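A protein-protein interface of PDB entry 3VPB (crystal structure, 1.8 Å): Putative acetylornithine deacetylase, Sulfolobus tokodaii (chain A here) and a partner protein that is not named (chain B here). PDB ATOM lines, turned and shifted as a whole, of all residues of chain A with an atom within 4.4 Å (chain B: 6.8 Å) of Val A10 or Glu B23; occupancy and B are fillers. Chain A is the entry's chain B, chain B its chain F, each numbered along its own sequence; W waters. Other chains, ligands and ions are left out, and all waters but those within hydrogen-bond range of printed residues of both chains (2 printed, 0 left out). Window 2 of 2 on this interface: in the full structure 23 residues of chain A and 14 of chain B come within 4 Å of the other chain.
Of the 15 printed residues of chain B, 6 touch a printed residue of chain A. Of the 7 printed residues of chain A, 4 touch a printed residue of chain B.
N of Val A10 lies within hydrogen-bond range of O of Gly B22, 2.9 Å away. The side-chain amino group of Lys A15 is in salt-bridge range of the side-chain carboxylate of Asp B18, 3.9 Å away. O of Asp A8 lies close to OE1 of Glu B34 (3.0 Å).
The side-chain carboxylate (OE2) of Glu B23 sits at hydrogen-bond distance from the backbone NH (N) of Leu B20, 2.7 Å away. The backbone NH of Gly B22 is in hydrogen-bond range of the backbone carbonyl oxygen of Val B35. The backbone NH of Val B35 is in hydrogen-bond range of the backbone carbonyl oxygen of Glu B23, 2.8 Å away.
Water W1 lies within hydrogen-bond range of OD2 of Asp B18 (2.7 Å) and NZ of Lys A15 (3.0 Å). Water W2 lies within hydrogen-bond range of O of Val A10 (2.7 Å) and N of Ile B24 (2.9 Å).
CA of Ile A9 touches O of Gly B22, 3.6 Å away. Ile B24 touches Ile A9. Glu B34 touches Ile A9. Val A10 touches Pro B21 (CG2 to O, 3.5 Å). Val A10 touches Glu B23 (O to CA, 3.5 Å). Glu B23 touches Lys A15 (OE2 to CD, 3.1 Å).
Of the printed residues of chain B, Val A10 touches Pro B21, Gly B22 and Glu B23. Printed residues of chain A within 4 Å of Asp B18: Lys A15. Of chain A, only Val A10 (3.5 Å) and Lys A15 (3.1 Å) come within 4 Å of Glu B23. Of the printed residues of chain A, Ile B24 touches Ile A9. The nearest printed residue of chain A that does not touch Glu B23 is Ile A9 (5.4 Å).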
ATOM      1  N   VAL A   7      20.069  16.872  17.539  1.00  0.00           N
ATOM      2  CA  VAL A   7      19.254  16.965  16.325  1.00  0.00           C
ATOM      3  C   VAL A   7      18.694  18.388  16.178  1.00  0.00           C
ATOM      4  O   VAL A   7      18.708  19.159  17.141  1.00  0.00           O
ATOM      5  CB  VAL A   7      18.062  15.959  16.381  1.00  0.00           C
ATOM      6  CG1 VAL A   7      18.579  14.515  16.628  1.00  0.00           C
ATOM      7  CG2 VAL A   7      17.021  16.360  17.457  1.00  0.00           C
ATOM      8  N   ASP A   8      18.251  18.746  14.974  1.00  0.00           N
ATOM      9  CA  ASP A   8      17.390  19.926  14.830  1.00  0.00           C
ATOM     10  C   ASP A   8      16.090  19.554  14.129  1.00  0.00           C
ATOM     11  O   ASP A   8      14.988  19.777  14.652  1.00  0.00           O
ATOM     12  CB  ASP A   8      18.109  21.155  14.206  1.00  0.00           C
ATOM     13  CG  ASP A   8      18.799  20.869  12.870  1.00  0.00           C
ATOM     14  OD1 ASP A   8      19.558  21.770  12.391  1.00  0.00           O
ATOM     15  OD2 ASP A   8      18.600  19.793  12.271  1.00  0.00           O
ATOM     16  N   ILE A   9      16.221  18.987  12.939  1.00  0.00           N
ATOM     17  CA  ILE A   9      15.078  18.399  12.261  1.00  0.00           C
ATOM     18  C   ILE A   9      15.284  16.892  12.293  1.00  0.00           C
ATOM     19  O   ILE A   9      16.360  16.405  11.949  1.00  0.00           O
ATOM     20  CB  ILE A   9      14.945  18.886  10.789  1.00  0.00           C
ATOM     21  CG1 ILE A   9      14.417  20.328  10.715  1.00  0.00           C
ATOM     22  CG2 ILE A   9      13.979  17.971  10.019  1.00  0.00           C
ATOM     23  CD1 ILE A   9      15.371  21.414  11.180  1.00  0.00           C
ATOM     24  N   VAL A  10      14.261  16.161  12.713  1.00  0.00           N
ATOM     25  CA  VAL A  10      14.331  14.711  12.814  1.00  0.00           C
ATOM     26  C   VAL A  10      13.857  14.079  11.501  1.00  0.00           C
ATOM     27  O   VAL A  10      12.658  14.131  11.171  1.00  0.00           O
ATOM     28  CB  VAL A  10      13.527  14.189  14.044  1.00  0.00           C
ATOM     29  CG1 VAL A  10      13.379  12.697  13.992  1.00  0.00           C
ATOM     30  CG2 VAL A  10      14.215  14.599  15.351  1.00  0.00           C
ATOM     31  N   ARG A  11      14.812  13.564  10.722  1.00  0.00           N
ATOM     32  CA  ARG A  11      14.510  12.841   9.481  1.00  0.00           C
ATOM     33  C   ARG A  11      14.467  11.348   9.762  1.00  0.00           C
ATOM     34  O   ARG A  11      14.753  10.899  10.887  1.00  0.00           O
ATOM     35  CB  ARG A  11      15.597  13.064   8.407  1.00  0.00           C
ATOM     36  CG  ARG A  11      15.954  14.489   8.091  1.00  0.00           C
ATOM     37  CD  ARG A  11      17.316  14.572   7.446  1.00  0.00           C
ATOM     38  NE  ARG A  11      18.389  14.496   8.448  1.00  0.00           N
ATOM     39  CZ  ARG A  11      19.628  14.932   8.260  1.00  0.00           C
ATOM     40  NH1 ARG A  11      19.959  15.467   7.090  1.00  0.00           N
ATOM     41  NH2 ARG A  11      20.528  14.858   9.252  1.00  0.00           N
ATOM     42  N   GLU A  14      17.556  10.101  11.602  1.00  0.00           N
ATOM     43  CA  GLU A  14      17.596  10.302  13.048  1.00  0.00           C
ATOM     44  C   GLU A  14      16.688   9.316  13.787  1.00  0.00           C
ATOM     45  O   GLU A  14      17.053   8.813  14.851  1.00  0.00           O
ATOM     46  CB  GLU A  14      17.261  11.741  13.416  1.00  0.00           C
ATOM     47  CG  GLU A  14      18.391  12.721  13.073  1.00  0.00           C
ATOM     48  CD  GLU A  14      18.580  12.934  11.557  1.00  0.00           C
ATOM     49  OE1 GLU A  14      17.580  13.153  10.840  1.00  0.00           O
ATOM     50  OE2 GLU A  14      19.731  12.890  11.087  1.00  0.00           O
ATOM     51  N   LYS A  15      15.527   9.032  13.207  1.00  0.00           N
ATOM     52  CA  LYS A  15      14.597   8.062  13.800  1.00  0.00           C
ATOM     53  C   LYS A  15      15.214   6.685  13.863  1.00  0.00           C
ATOM     54  O   LYS A  15      15.114   5.986  14.899  1.00  0.00           O
ATOM     55  CB  LYS A  15      13.295   8.027  13.009  1.00  0.00           C
ATOM     56  CG  LYS A  15      12.481   9.277  13.193  1.00  0.00           C
ATOM     57  CD  LYS A  15      11.195   9.213  12.370  1.00  0.00           C
ATOM     58  CE  LYS A  15      11.488   9.262  10.892  1.00  0.00           C
ATOM     59  NZ  LYS A  15      10.406   8.570  10.131  1.00  0.00           N
ATOM     60  N   VAL B  15      -1.437  13.322  12.861  1.00  0.00           N
ATOM     61  CA  VAL B  15      -0.028  13.029  13.092  1.00  0.00           C
ATOM     62  C   VAL B  15       0.134  11.564  13.534  1.00  0.00           C
ATOM     63  O   VAL B  15      -0.494  11.145  14.510  1.00  0.00           O
ATOM     64  CB  VAL B  15       0.552  14.021  14.131  1.00  0.00           C
ATOM     65  CG1 VAL B  15       1.984  13.671  14.516  1.00  0.00           C
ATOM     66  CG2 VAL B  15       0.466  15.445  13.598  1.00  0.00           C
ATOM     67  N   PRO B  16       0.970  10.778  12.815  1.00  0.00           N
ATOM     68  CA  PRO B  16       1.145   9.334  13.112  1.00  0.00           C
ATOM     69  C   PRO B  16       1.693   9.022  14.523  1.00  0.00           C
ATOM     70  O   PRO B  16       2.231   9.910  15.187  1.00  0.00           O
ATOM     71  CB  PRO B  16       2.137   8.871  12.037  1.00  0.00           C
ATOM     72  CG  PRO B  16       2.850  10.115  11.592  1.00  0.00           C
ATOM     73  CD  PRO B  16       1.809  11.206  11.679  1.00  0.00           C
ATOM     74  N   ASP B  18       4.129   7.008  14.972  1.00  0.00           N
ATOM     75  CA  ASP B  18       5.559   7.029  14.666  1.00  0.00           C
ATOM     76  C   ASP B  18       6.203   8.299  15.245  1.00  0.00           C
ATOM     77  O   ASP B  18       7.304   8.250  15.810  1.00  0.00           O
ATOM     78  CB  ASP B  18       5.726   6.972  13.136  1.00  0.00           C
ATOM     79  CG  ASP B  18       7.171   7.150  12.677  1.00  0.00           C
ATOM     80  OD1 ASP B  18       7.804   8.185  13.004  1.00  0.00           O
ATOM     81  OD2 ASP B  18       7.664   6.259  11.950  1.00  0.00           O
ATOM     82  N   ALA B  19       5.471   9.412  15.125  1.00  0.00           N
ATOM     83  CA  ALA B  19       5.973  10.779  15.311  1.00  0.00           C
ATOM     84  C   ALA B  19       6.859  11.050  16.516  1.00  0.00           C
ATOM     85  O   ALA B  19       6.467  10.846  17.664  1.00  0.00           O
ATOM     86  CB  ALA B  19       4.818  11.764  15.300  1.00  0.00           C
ATOM     87  N   LEU B  20       8.060  11.526  16.220  1.00  0.00           N
ATOM     88  CA  LEU B  20       8.976  12.043  17.216  1.00  0.00           C
ATOM     89  C   LEU B  20       8.908  13.564  17.170  1.00  0.00           C
ATOM     90  O   LEU B  20       8.686  14.146  16.099  1.00  0.00           O
ATOM     91  CB  LEU B  20      10.414  11.591  16.920  1.00  0.00           C
ATOM     92  CG  LEU B  20      10.955  10.292  17.519  1.00  0.00           C
ATOM     93  CD1 LEU B  20      10.540   9.078  16.692  1.00  0.00           C
ATOM     94  CD2 LEU B  20      12.475  10.370  17.641  1.00  0.00           C
ATOM     95  N   PRO B  21       9.090  14.222  18.331  1.00  0.00           N
ATOM     96  CA  PRO B  21       9.270  15.674  18.268  1.00  0.00           C
ATOM     97  C   PRO B  21      10.466  16.013  17.362  1.00  0.00           C
ATOM     98  O   PRO B  21      11.496  15.327  17.424  1.00  0.00           O
ATOM     99  CB  PRO B  21       9.535  16.060  19.728  1.00  0.00           C
ATOM    100  CG  PRO B  21       8.925  14.949  20.535  1.00  0.00           C
ATOM    101  CD  PRO B  21       9.039  13.709  19.714  1.00  0.00           C
ATOM    102  N   GLY B  22      10.306  17.026  16.506  1.00  0.00           N
ATOM    103  CA  GLY B  22      11.332  17.420  15.520  1.00  0.00           C
ATOM    104  C   GLY B  22      11.072  16.972  14.082  1.00  0.00           C
ATOM    105  O   GLY B  22      11.698  17.474  13.147  1.00  0.00           O
ATOM    106  N   GLU B  23      10.159  16.021  13.903  1.00  0.00           N
ATOM    107  CA  GLU B  23       9.761  15.556  12.575  1.00  0.00           C
ATOM    108  C   GLU B  23       8.922  16.600  11.844  1.00  0.00           C
ATOM    109  O   GLU B  23       8.202  17.378  12.466  1.00  0.00           O
ATOM    110  CB  GLU B  23       8.941  14.273  12.667  1.00  0.00           C
ATOM    111  CG  GLU B  23       9.706  13.012  13.027  1.00  0.00           C
ATOM    112  CD  GLU B  23       8.802  11.787  13.027  1.00  0.00           C
ATOM    113  OE1 GLU B  23       7.841  11.748  12.230  1.00  0.00           O
ATOM    114  OE2 GLU B  23       9.045  10.867  13.827  1.00  0.00           O
ATOM    115  N   ILE B  24       9.031  16.596  10.520  1.00  0.00           N
ATOM    116  CA  ILE B  24       8.322  17.543   9.669  1.00  0.00           C
ATOM    117  C   ILE B  24       7.072  16.897   9.103  1.00  0.00           C
ATOM    118  O   ILE B  24       7.087  15.708   8.747  1.00  0.00           O
ATOM    119  CB  ILE B  24       9.246  18.044   8.520  1.00  0.00           C
ATOM    120  CG1 ILE B  24      10.504  18.704   9.088  1.00  0.00           C
ATOM    121  CG2 ILE B  24       8.523  19.028   7.598  1.00  0.00           C
ATOM    122  CD1 ILE B  24      10.241  19.917   9.997  1.00  0.00           C
ATOM    123  N   VAL B  25       5.982  17.668   9.044  1.00  0.00           N
ATOM    124  CA  VAL B  25       4.756  17.211   8.392  1.00  0.00           C
ATOM    125  C   VAL B  25       4.214  18.329   7.496  1.00  0.00           C
ATOM    126  O   VAL B  25       4.212  19.499   7.886  1.00  0.00           O
ATOM    127  CB  VAL B  25       3.648  16.739   9.405  1.00  0.00           C
ATOM    128  CG1 VAL B  25       4.134  15.569  10.282  1.00  0.00           C
ATOM    129  CG2 VAL B  25       3.161  17.881  10.278  1.00  0.00           C
ATOM    130  N   LEU B  33       5.200  22.060   8.673  1.00  0.00           N
ATOM    131  CA  LEU B  33       5.049  22.158  10.128  1.00  0.00           C
ATOM    132  C   LEU B  33       6.081  21.237  10.775  1.00  0.00           C
ATOM    133  O   LEU B  33       6.533  20.309  10.131  1.00  0.00           O
ATOM    134  CB  LEU B  33       3.644  21.714  10.542  1.00  0.00           C
ATOM    135  CG  LEU B  33       2.491  22.392   9.792  1.00  0.00           C
ATOM    136  CD1 LEU B  33       1.160  21.704  10.073  1.00  0.00           C
ATOM    137  CD2 LEU B  33       2.457  23.894  10.126  1.00  0.00           C
ATOM    138  N   GLU B  34       6.462  21.520  12.020  1.00  0.00           N
ATOM    139  CA  GLU B  34       7.386  20.668  12.776  1.00  0.00           C
ATOM    140  C   GLU B  34       6.689  20.223  14.055  1.00  0.00           C
ATOM    141  O   GLU B  34       6.067  21.039  14.721  1.00  0.00           O
ATOM    142  CB  GLU B  34       8.679  21.422  13.118  1.00  0.00           C
ATOM    143  CG  GLU B  34       9.809  20.513  13.723  1.00  0.00           C
ATOM    144  CD  GLU B  34      11.233  20.925  13.304  1.00  0.00           C
ATOM    145  OE1 GLU B  34      12.208  20.283  13.774  1.00  0.00           O
ATOM    146  OE2 GLU B  34      11.389  21.869  12.500  1.00  0.00           O
ATOM    147  N   VAL B  35       6.806  18.938  14.390  1.00  0.00           N
ATOM    148  CA  VAL B  35       6.271  18.421  15.663  1.00  0.00           C
ATOM    149  C   VAL B  35       7.151  18.912  16.823  1.00  0.00           C
ATOM    150  O   VAL B  35       8.393  18.877  16.726  1.00  0.00           O
ATOM    151  CB  VAL B  35       6.211  16.856  15.687  1.00  0.00           C
ATOM    152  CG1 VAL B  35       5.566  16.344  16.997  1.00  0.00           C
ATOM    153  CG2 VAL B  35       5.477  16.293  14.459  1.00  0.00           C
ATOM    154  N   TYR B  36       6.521  19.357  17.916  1.00  0.00           N
ATOM    155  CA  TYR B  36       7.269  19.716  19.121  1.00  0.00           C
ATOM    156  C   TYR B  36       6.492  19.312  20.370  1.00  0.00           C
ATOM    157  O   TYR B  36       5.306  19.029  20.290  1.00  0.00           O
ATOM    158  CB  TYR B  36       7.683  21.203  19.140  1.00  0.00           C
ATOM    159  CG  TYR B  36       6.574  22.190  19.463  1.00  0.00           C
ATOM    160  CD1 TYR B  36       6.455  22.741  20.750  1.00  0.00           C
ATOM    161  CD2 TYR B  36       5.671  22.597  18.486  1.00  0.00           C
ATOM    162  CE1 TYR B  36       5.441  23.647  21.063  1.00  0.00           C
ATOM    163  CE2 TYR B  36       4.649  23.519  18.786  1.00  0.00           C
ATOM    164  CZ  TYR B  36       4.553  24.039  20.079  1.00  0.00           C
ATOM    165  OH  TYR B  36       3.555  24.933  20.384  1.00  0.00           O
ATOM    166  N   LEU B  44       2.102  21.534  16.950  1.00  0.00           N
ATOM    167  CA  LEU B  44       2.721  21.832  15.665  1.00  0.00           C
ATOM    168  C   LEU B  44       3.066  23.310  15.574  1.00  0.00           C
ATOM    169  O   LEU B  44       2.236  24.151  15.920  1.00  0.00           O
ATOM    170  CB  LEU B  44       1.773  21.433  14.544  1.00  0.00           C
ATOM    171  CG  LEU B  44       1.442  19.948  14.376  1.00  0.00           C
ATOM    172  CD1 LEU B  44       0.242  19.756  13.479  1.00  0.00           C
ATOM    173  CD2 LEU B  44       2.665  19.186  13.824  1.00  0.00           C
HETATM  174  O   HOH W   1       9.281   5.796   9.798  1.00  0.00           O
HETATM  175  O   HOH W   2      10.953  14.885   9.168  1.00  0.00           O
